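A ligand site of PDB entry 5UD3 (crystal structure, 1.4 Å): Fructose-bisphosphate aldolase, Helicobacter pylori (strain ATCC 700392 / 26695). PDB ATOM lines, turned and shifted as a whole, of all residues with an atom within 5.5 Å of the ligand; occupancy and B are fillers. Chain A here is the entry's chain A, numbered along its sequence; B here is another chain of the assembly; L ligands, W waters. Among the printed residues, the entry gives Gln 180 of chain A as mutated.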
ATOM      1  N   ASN A  23      -3.142 -25.919 -14.457  1.00  0.00           N
ATOM      2  CA  ASN A  23      -4.284 -25.954 -15.358  1.00  0.00           C
ATOM      3  C   ASN A  23      -5.474 -26.623 -14.681  1.00  0.00           C
ATOM      4  O   ASN A  23      -5.319 -27.503 -13.836  1.00  0.00           O
ATOM      5  CB  ASN A  23      -3.946 -26.749 -16.609  1.00  0.00           C
ATOM      6  CG  ASN A  23      -3.070 -25.982 -17.548  1.00  0.00           C
ATOM      7  OD1 ASN A  23      -1.858 -25.973 -17.399  1.00  0.00           O
ATOM      8  ND2 ASN A  23      -3.691 -25.312 -18.526  1.00  0.00           N
ATOM      9  N   VAL A  25      -9.767 -27.977 -15.693  1.00  0.00           N
ATOM     10  CA  VAL A  25     -10.847 -28.164 -16.660  1.00  0.00           C
ATOM     11  C   VAL A  25     -12.212 -28.277 -16.004  1.00  0.00           C
ATOM     12  O   VAL A  25     -13.223 -28.346 -16.712  1.00  0.00           O
ATOM     13  CB  VAL A  25     -10.611 -29.353 -17.610  1.00  0.00           C
ATOM     14  CG1 VAL A  25      -9.228 -29.269 -18.243  1.00  0.00           C
ATOM     15  CG2 VAL A  25     -10.858 -30.695 -16.937  1.00  0.00           C
ATOM     16  N   GLN A  47      -4.740 -21.541 -14.437  1.00  0.00           N
ATOM     17  CA  GLN A  47      -4.756 -21.307 -15.873  1.00  0.00           C
ATOM     18  C   GLN A  47      -5.696 -22.265 -16.595  1.00  0.00           C
ATOM     19  O   GLN A  47      -5.961 -23.388 -16.155  1.00  0.00           O
ATOM     20  CB  GLN A  47      -3.350 -21.234 -16.494  1.00  0.00           C
ATOM     21  CG  GLN A  47      -2.478 -22.450 -16.336  1.00  0.00           C
ATOM     22  CD  GLN A  47      -1.117 -22.283 -17.021  1.00  0.00           C
ATOM     23  OE1 GLN A  47      -0.565 -21.181 -17.117  1.00  0.00           O
ATOM     24  NE2 GLN A  47      -0.579 -23.383 -17.499  1.00  0.00           N
ATOM     25  N   SER A  49      -6.556 -23.464 -20.638  1.00  0.00           N
ATOM     26  CA  SER A  49      -6.284 -23.481 -22.067  1.00  0.00           C
ATOM     27  C   SER A  49      -7.545 -23.127 -22.856  1.00  0.00           C
ATOM     28  O   SER A  49      -8.659 -23.078 -22.324  1.00  0.00           O
ATOM     29  CB  SER A  49      -5.839 -24.875 -22.473  1.00  0.00           C
ATOM     30  OG  SER A  49      -6.924 -25.776 -22.321  1.00  0.00           O
ATOM     31  N   GLY A  51      -8.911 -25.039 -25.016  1.00  0.00           N
ATOM     32  CA  GLY A  51      -9.760 -26.222 -24.979  1.00  0.00           C
ATOM     33  C   GLY A  51     -10.517 -26.355 -23.672  1.00  0.00           C
ATOM     34  O   GLY A  51     -11.682 -26.764 -23.661  1.00  0.00           O
ATOM     35  N   ALA A  52      -9.861 -26.020 -22.557  1.00  0.00           N
ATOM     36  CA  ALA A  52     -10.559 -26.028 -21.270  1.00  0.00           C
ATOM     37  C   ALA A  52     -11.676 -25.001 -21.253  1.00  0.00           C
ATOM     38  O   ALA A  52     -12.760 -25.259 -20.725  1.00  0.00           O
ATOM     39  CB  ALA A  52      -9.555 -25.747 -20.157  1.00  0.00           C
ATOM     40  N   ASP A  82      -4.026 -19.744 -20.908  1.00  0.00           N
ATOM     41  CA  ASP A  82      -2.840 -20.503 -21.315  1.00  0.00           C
ATOM     42  C   ASP A  82      -2.895 -20.782 -22.810  1.00  0.00           C
ATOM     43  O   ASP A  82      -3.882 -21.312 -23.319  1.00  0.00           O
ATOM     44  CB  ASP A  82      -2.838 -21.793 -20.508  1.00  0.00           C
ATOM     45  CG  ASP A  82      -1.681 -22.704 -20.822  1.00  0.00           C
ATOM     46  OD1 ASP A  82      -0.613 -22.221 -21.256  1.00  0.00           O
ATOM     47  OD2 ASP A  82      -1.866 -23.926 -20.596  1.00  0.00           O
ATOM     48  N   HIS A  83      -1.834 -20.408 -23.519  1.00  0.00           N
ATOM     49  CA  HIS A  83      -1.691 -20.666 -24.946  1.00  0.00           C
ATOM     50  C   HIS A  83      -2.870 -20.152 -25.753  1.00  0.00           C
ATOM     51  O   HIS A  83      -3.505 -20.872 -26.533  1.00  0.00           O
ATOM     52  CB  HIS A  83      -1.396 -22.139 -25.235  1.00  0.00           C
ATOM     53  CG  HIS A  83       0.041 -22.489 -24.982  1.00  0.00           C
ATOM     54  ND1 HIS A  83       0.531 -22.704 -23.709  1.00  0.00           N
ATOM     55  CD2 HIS A  83       1.096 -22.589 -25.817  1.00  0.00           C
ATOM     56  CE1 HIS A  83       1.827 -22.959 -23.782  1.00  0.00           C
ATOM     57  NE2 HIS A  83       2.189 -22.890 -25.051  1.00  0.00           N
ATOM     58  N   SER A 179       8.929 -29.715 -23.607  1.00  0.00           N
ATOM     59  CA  SER A 179       7.772 -29.888 -24.485  1.00  0.00           C
ATOM     60  C   SER A 179       6.618 -30.328 -23.607  1.00  0.00           C
ATOM     61  O   SER A 179       6.821 -30.771 -22.470  1.00  0.00           O
ATOM     62  CB  SER A 179       8.034 -30.903 -25.592  1.00  0.00           C
ATOM     63  OG  SER A 179       8.459 -32.146 -25.066  1.00  0.00           O
ATOM     64  N   GLN A 180       5.406 -30.217 -24.144  1.00  0.00           N
ATOM     65  CA  GLN A 180       4.215 -30.564 -23.366  1.00  0.00           C
ATOM     66  C   GLN A 180       3.985 -32.071 -23.362  1.00  0.00           C
ATOM     67  O   GLN A 180       4.411 -32.809 -24.256  1.00  0.00           O
ATOM     68  CB  GLN A 180       2.961 -29.889 -23.925  1.00  0.00           C
ATOM     69  CG  GLN A 180       2.662 -28.535 -23.312  1.00  0.00           C
ATOM     70  CD  GLN A 180       3.721 -27.510 -23.611  1.00  0.00           C
ATOM     71  OE1 GLN A 180       4.846 -27.591 -23.111  1.00  0.00           O
ATOM     72  NE2 GLN A 180       3.389 -26.530 -24.451  1.00  0.00           N
ATOM     73  N   GLY A 181       3.271 -32.528 -22.338  1.00  0.00           N
ATOM     74  CA  GLY A 181       2.829 -33.908 -22.280  1.00  0.00           C
ATOM     75  C   GLY A 181       3.766 -34.816 -21.504  1.00  0.00           C
ATOM     76  O   GLY A 181       4.767 -34.404 -20.908  1.00  0.00           O
ATOM     77  N   ALA A 182       3.422 -36.104 -21.528  1.00  0.00           N
ATOM     78  CA  ALA A 182       4.118 -37.093 -20.717  1.00  0.00           C
ATOM     79  C   ALA A 182       5.400 -37.638 -21.353  1.00  0.00           C
ATOM     80  O   ALA A 182       6.115 -38.389 -20.693  1.00  0.00           O
ATOM     81  CB  ALA A 182       3.187 -38.262 -20.382  1.00  0.00           C
ATOM     82  N   LYS A 184       8.445 -36.193 -22.828  1.00  0.00           N
ATOM     83  CA  LYS A 184       9.258 -35.006 -23.111  1.00  0.00           C
ATOM     84  C   LYS A 184      10.627 -35.365 -23.680  1.00  0.00           C
ATOM     85  O   LYS A 184      11.153 -34.613 -24.500  1.00  0.00           O
ATOM     86  CB  LYS A 184       9.442 -34.192 -21.836  1.00  0.00           C
ATOM     87  CG  LYS A 184       8.127 -33.806 -21.159  1.00  0.00           C
ATOM     88  CD  LYS A 184       8.374 -32.876 -19.993  1.00  0.00           C
ATOM     89  CE  LYS A 184       7.079 -32.596 -19.209  1.00  0.00           C
ATOM     90  NZ  LYS A 184       5.991 -32.025 -20.064  1.00  0.00           N
ATOM     91  N   LEU A 209       8.335 -21.300 -17.588  1.00  0.00           N
ATOM     92  CA  LEU A 209       8.716 -22.625 -18.061  1.00  0.00           C
ATOM     93  C   LEU A 209       7.446 -23.372 -18.467  1.00  0.00           C
ATOM     94  O   LEU A 209       6.581 -23.632 -17.631  1.00  0.00           O
ATOM     95  CB  LEU A 209       9.451 -23.409 -16.985  1.00  0.00           C
ATOM     96  CG  LEU A 209      10.092 -24.718 -17.472  1.00  0.00           C
ATOM     97  CD1 LEU A 209      11.222 -24.432 -18.434  1.00  0.00           C
ATOM     98  CD2 LEU A 209      10.593 -25.547 -16.285  1.00  0.00           C
ATOM     99  N   HIS A 210       7.347 -23.721 -19.738  1.00  0.00           N
ATOM    100  CA  HIS A 210       6.282 -24.578 -20.237  1.00  0.00           C
ATOM    101  C   HIS A 210       6.698 -26.041 -20.142  1.00  0.00           C
ATOM    102  O   HIS A 210       7.880 -26.374 -20.049  1.00  0.00           O
ATOM    103  CB  HIS A 210       5.981 -24.272 -21.698  1.00  0.00           C
ATOM    104  CG  HIS A 210       5.386 -22.920 -21.916  1.00  0.00           C
ATOM    105  ND1 HIS A 210       5.223 -22.385 -23.177  1.00  0.00           N
ATOM    106  CD2 HIS A 210       4.918 -21.990 -21.050  1.00  0.00           C
ATOM    107  CE1 HIS A 210       4.680 -21.183 -23.074  1.00  0.00           C
ATOM    108  NE2 HIS A 210       4.464 -20.935 -21.790  1.00  0.00           N
ATOM    109  N   GLY A 211       5.698 -26.920 -20.168  1.00  0.00           N
ATOM    110  CA  GLY A 211       5.969 -28.349 -20.183  1.00  0.00           C
ATOM    111  C   GLY A 211       6.794 -28.799 -18.990  1.00  0.00           C
ATOM    112  O   GLY A 211       7.743 -29.574 -19.142  1.00  0.00           O
ATOM    113  N   ALA A 212       6.411 -28.341 -17.810  1.00  0.00           N
ATOM    114  CA  ALA A 212       7.220 -28.503 -16.609  1.00  0.00           C
ATOM    115  C   ALA A 212       6.751 -29.628 -15.698  1.00  0.00           C
ATOM    116  O   ALA A 212       7.220 -29.705 -14.552  1.00  0.00           O
ATOM    117  CB  ALA A 212       7.267 -27.181 -15.841  1.00  0.00           C
ATOM    118  N   SER A 213       5.860 -30.511 -16.143  1.00  0.00           N
ATOM    119  CA  SER A 213       5.505 -31.645 -15.305  1.00  0.00           C
ATOM    120  C   SER A 213       6.712 -32.550 -15.105  1.00  0.00           C
ATOM    121  O   SER A 213       7.573 -32.667 -15.978  1.00  0.00           O
ATOM    122  CB  SER A 213       4.336 -32.425 -15.887  1.00  0.00           C
ATOM    123  OG  SER A 213       3.112 -31.800 -15.567  1.00  0.00           O
ATOM    124  N   ASN A 253       4.525 -24.023 -15.571  1.00  0.00           N
ATOM    125  CA  ASN A 253       3.265 -24.541 -16.080  1.00  0.00           C
ATOM    126  C   ASN A 253       3.165 -26.038 -15.838  1.00  0.00           C
ATOM    127  O   ASN A 253       4.003 -26.807 -16.323  1.00  0.00           O
ATOM    128  CB  ASN A 253       3.181 -24.284 -17.583  1.00  0.00           C
ATOM    129  CG  ASN A 253       2.889 -22.832 -17.919  1.00  0.00           C
ATOM    130  OD1 ASN A 253       3.203 -21.925 -17.155  1.00  0.00           O
ATOM    131  ND2 ASN A 253       2.264 -22.613 -19.078  1.00  0.00           N
ATOM    132  N   THR A 254       2.104 -26.462 -15.142  1.00  0.00           N
ATOM    133  CA  THR A 254       1.975 -27.837 -14.663  1.00  0.00           C
ATOM    134  C   THR A 254       0.548 -28.314 -14.901  1.00  0.00           C
ATOM    135  O   THR A 254      -0.399 -27.740 -14.355  1.00  0.00           O
ATOM    136  CB  THR A 254       2.332 -27.891 -13.183  1.00  0.00           C
ATOM    137  OG1 THR A 254       3.589 -27.235 -12.983  1.00  0.00           O
ATOM    138  CG2 THR A 254       2.461 -29.314 -12.688  1.00  0.00           C
ATOM    139  N   ASP A 255       0.394 -29.385 -15.698  1.00  0.00           N
ATOM    140  CA  ASP A 255      -0.913 -29.919 -16.068  1.00  0.00           C
ATOM    141  C   ASP A 255      -0.898 -31.445 -16.062  1.00  0.00           C
ATOM    142  O   ASP A 255      -1.665 -32.084 -15.340  1.00  0.00           O
ATOM    143  CB  ASP A 255      -1.326 -29.350 -17.447  1.00  0.00           C
ATOM    144  CG  ASP A 255      -2.784 -29.666 -17.839  1.00  0.00           C
ATOM    145  OD1 ASP A 255      -3.434 -30.497 -17.176  1.00  0.00           O
ATOM    146  OD2 ASP A 255      -3.273 -29.086 -18.846  1.00  0.00           O
ATOM    147  N   THR A 256       0.033 -32.030 -16.821  1.00  0.00           N
ATOM    148  CA  THR A 256       0.091 -33.482 -16.962  1.00  0.00           C
ATOM    149  C   THR A 256       0.161 -34.203 -15.614  1.00  0.00           C
ATOM    150  O   THR A 256      -0.538 -35.188 -15.395  1.00  0.00           O
ATOM    151  CB  THR A 256       1.285 -33.856 -17.859  1.00  0.00           C
ATOM    152  OG1 THR A 256       1.077 -33.331 -19.177  1.00  0.00           O
ATOM    153  CG2 THR A 256       1.469 -35.377 -17.938  1.00  0.00           C
ATOM    154  N   ASP A 257       1.025 -33.735 -14.705  1.00  0.00           N
ATOM    155  CA  ASP A 257       1.134 -34.382 -13.404  1.00  0.00           C
ATOM    156  C   ASP A 257      -0.209 -34.416 -12.700  1.00  0.00           C
ATOM    157  O   ASP A 257      -0.531 -35.402 -12.022  1.00  0.00           O
ATOM    158  CB  ASP A 257       2.141 -33.646 -12.502  1.00  0.00           C
ATOM    159  CG  ASP A 257       3.580 -33.923 -12.869  1.00  0.00           C
ATOM    160  OD1 ASP A 257       3.841 -34.824 -13.698  1.00  0.00           O
ATOM    161  OD2 ASP A 257       4.459 -33.242 -12.307  1.00  0.00           O
ATOM    162  N   ARG A 259      -3.259 -34.386 -14.141  1.00  0.00           N
ATOM    163  CA  ARG A 259      -4.152 -35.316 -14.828  1.00  0.00           C
ATOM    164  C   ARG A 259      -3.854 -36.751 -14.450  1.00  0.00           C
ATOM    165  O   ARG A 259      -4.769 -37.553 -14.205  1.00  0.00           O
ATOM    166  CB  ARG A 259      -3.985 -35.163 -16.335  1.00  0.00           C
ATOM    167  CG  ARG A 259      -4.321 -33.827 -16.908  1.00  0.00           C
ATOM    168  CD  ARG A 259      -4.188 -33.900 -18.421  1.00  0.00           C
ATOM    169  NE  ARG A 259      -4.124 -32.585 -19.037  1.00  0.00           N
ATOM    170  CZ  ARG A 259      -4.207 -32.347 -20.345  1.00  0.00           C
ATOM    171  NH1 ARG A 259      -4.390 -33.335 -21.213  1.00  0.00           N
ATOM    172  NH2 ARG A 259      -4.121 -31.103 -20.789  1.00  0.00           N
ATOM    173  N   ASP B 278      -6.677 -37.432 -20.061  1.00  0.00           N
ATOM    174  CA  ASP B 278      -7.343 -36.146 -20.229  1.00  0.00           C
ATOM    175  C   ASP B 278      -8.740 -36.255 -19.646  1.00  0.00           C
ATOM    176  O   ASP B 278      -9.555 -37.050 -20.132  1.00  0.00           O
ATOM    177  CB  ASP B 278      -7.415 -35.786 -21.711  1.00  0.00           C
ATOM    178  CG  ASP B 278      -7.979 -34.400 -21.963  1.00  0.00           C
ATOM    179  OD1 ASP B 278      -8.684 -33.838 -21.097  1.00  0.00           O
ATOM    180  OD2 ASP B 278      -7.721 -33.867 -23.058  1.00  0.00           O
ATOM    181  N   ARG B 280     -11.277 -34.494 -19.884  1.00  0.00           N
ATOM    182  CA  ARG B 280     -12.351 -34.166 -20.810  1.00  0.00           C
ATOM    183  C   ARG B 280     -12.715 -35.369 -21.685  1.00  0.00           C
ATOM    184  O   ARG B 280     -13.863 -35.492 -22.117  1.00  0.00           O
ATOM    185  CB  ARG B 280     -11.943 -32.987 -21.681  1.00  0.00           C
ATOM    186  CG  ARG B 280     -11.732 -31.705 -20.889  1.00  0.00           C
ATOM    187  CD  ARG B 280     -10.900 -30.699 -21.679  1.00  0.00           C
ATOM    188  NE  ARG B 280      -9.518 -31.162 -21.854  1.00  0.00           N
ATOM    189  CZ  ARG B 280      -8.469 -30.382 -22.137  1.00  0.00           C
ATOM    190  NH1 ARG B 280      -8.618 -29.078 -22.290  1.00  0.00           N
ATOM    191  NH2 ARG B 280      -7.269 -30.921 -22.268  1.00  0.00           N
HETATM  192  P1  LIG L   1       2.989 -30.300 -18.856  1.00  0.00           P
HETATM  193  O1  LIG L   1       2.174 -30.338 -17.585  1.00  0.00           O
HETATM  194  O2  LIG L   1       2.373 -31.027 -20.027  1.00  0.00           O
HETATM  195  O3  LIG L   1       4.441 -30.628 -18.630  1.00  0.00           O
HETATM  196  O4  LIG L   1       3.014 -28.728 -19.281  1.00  0.00           O
HETATM  197  C1  LIG L   1       1.891 -27.872 -19.094  1.00  0.00           C
HETATM  198  C2  LIG L   1       1.870 -26.740 -20.107  1.00  0.00           C
HETATM  199  O5  LIG L   1       2.890 -26.129 -20.439  1.00  0.00           O
HETATM  200  C3  LIG L   1       0.546 -26.090 -20.342  1.00  0.00           C
HETATM  201  O6  LIG L   1       0.701 -24.665 -20.448  1.00  0.00           O
HETATM  202  C4  LIG L   1      -0.094 -26.662 -21.616  1.00  0.00           C
HETATM  203  O7  LIG L   1      -0.122 -25.682 -22.654  1.00  0.00           O
HETATM  204  C5  LIG L   1      -1.511 -27.122 -21.334  1.00  0.00           C
HETATM  205  O8  LIG L   1      -1.347 -28.205 -20.436  1.00  0.00           O
HETATM  206  C6  LIG L   1      -2.268 -27.609 -22.563  1.00  0.00           C
HETATM  207  O9  LIG L   1      -3.590 -27.933 -22.153  1.00  0.00           O
HETATM  208  P2  LIG L   1      -4.744 -28.406 -23.187  1.00  0.00           P
HETATM  209  O10 LIG L   1      -4.577 -29.888 -23.410  1.00  0.00           O
HETATM  210  O11 LIG L   1      -4.481 -27.607 -24.447  1.00  0.00           O
HETATM  211  O12 LIG L   1      -6.006 -28.079 -22.426  1.00  0.00           O
HETATM  212  O   HOH W   1       0.425 -26.387 -25.204  1.00  0.00           O
HETATM  213  O   HOH W   2      -6.550 -26.581 -25.794  1.00  0.00           O
HETATM  214  O   HOH W   3      -5.914 -28.254 -19.613  1.00  0.00           O
HETATM  215  O   HOH W   4       0.050 -30.699 -21.391  1.00  0.00           O
HETATM  216  O   HOH W   5      -5.692 -31.333 -25.376  1.00  0.00           O
HETATM  217  O   HOH W   6      -3.181 -25.280 -24.993  1.00  0.00           O
HETATM  218  O   HOH W   7      -3.122 -28.770 -26.400  1.00  0.00           O
HETATM  219  O   HOH W   8      -3.326 -32.117 -24.083  1.00  0.00           O
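The side-chain hydroxyl of Ser 49 sits at hydrogen-bond distance from an oxygen (O12) of the ligand. An oxygen (O3) of the ligand is in salt-bridge range of the side-chain amino group (NZ) of Lys 184, 2.5 Å away. N of Asp 255 sits at hydrogen-bond distance from O1 of the ligand, 2.8 Å away. O8 of the ligand sits at hydrogen-bond distance from OD2 of Asp 255 (2.6 Å). An oxygen (O3) of the ligand sits at hydrogen-bond distance from the backbone NH (N) of Ser 213. An oxygen (O1) of the ligand is in hydrogen-bond range of the side-chain hydroxyl (OG) of Ser 213 (2.7 Å). The side-chain carboxylate of Asp 82 lies within hydrogen-bond range of an oxygen (O6) of the ligand. An oxygen (O1) of the ligand lies within hydrogen-bond range of the backbone NH of Thr 256 (2.8 Å). O2 of the ligand lies within hydrogen-bond range of OG1 of Thr 256 (2.8 Å). NH1 of Arg 280 of chain B is in salt-bridge range of O12 of the ligand. N of Gly 181 lies within hydrogen-bond range of O2 of the ligand (2.9 Å). The side-chain amide nitrogen (ND2) of Asn 253 sits at hydrogen-bond distance from an oxygen (O6) of the ligand (2.9 Å). An oxygen (O10) of the ligand is in salt-bridge range of the guanidinium group of Arg 259, 2.9 Å away. O5 of the ligand sits at hydrogen-bond distance from N of Gly 211 (2.9 Å). The backbone NH (N) of Ala 212 sits at hydrogen-bond distance from an oxygen (O3) of the ligand, at 3.1 Å. O7 of the ligand sits at hydrogen-bond distance from ND1 of His 83, 3.2 Å away. The side-chain amide nitrogen of Gln 47 sits at hydrogen-bond distance from an oxygen (O6) of the ligand (3.5 Å).
OG of Ser 49 sits at hydrogen-bond distance from N of Ala 52, 3.0 Å away. NZ of Lys 184 sits at hydrogen-bond distance from O of Ser 179 (2.8 Å). The guanidinium group (NE) of Arg 259 lies within salt-bridge range of the side-chain carboxylate (OD1) of Asp 255 (2.9 Å). The side-chain hydroxyl (OG) of Ser 213 sits at hydrogen-bond distance from the backbone NH (N) of Thr 256 (3.3 Å). The side-chain amide nitrogen of Asn 23 sits at hydrogen-bond distance from the side-chain carboxylate of Asp 82 (3.1 Å). The side-chain amide nitrogen of Asn 253 sits close to the side-chain amide nitrogen of Gln 47, 3.3 Å away. The backbone NH (N) of Asn 253 is in hydrogen-bond range of the backbone carbonyl oxygen (O) of Leu 209, at 2.9 Å. The backbone carbonyl oxygen of Thr 254 lies within hydrogen-bond range of the backbone NH of Asn 23 (3.3 Å).
Asn 23 touches the ligand. Gln 180 touches the ligand. CA of His 210 touches O5 of the ligand, at 3.7 Å. Thr 254 touches the ligand (C to O1, 3.7 Å). Hydrophobic or aromatic side chains that line the ligand: His 83 and His 210.
Water W8 bridges O10 of the ligand and NH1 of Arg 259. Water W2 lies within hydrogen-bond range of an oxygen (O11) of the ligand (2.7 Å) and the backbone NH (N) of Gly 51 (2.9 Å). Water W1 bridges O7 of the ligand (2.7 Å) and NE2 of Gln 180 (3.1 Å). Water W3 lies within hydrogen-bond range of an oxygen (O12) of the ligand (2.8 Å) and the side-chain carboxylate (OD2) of Asp 255 (2.9 Å).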
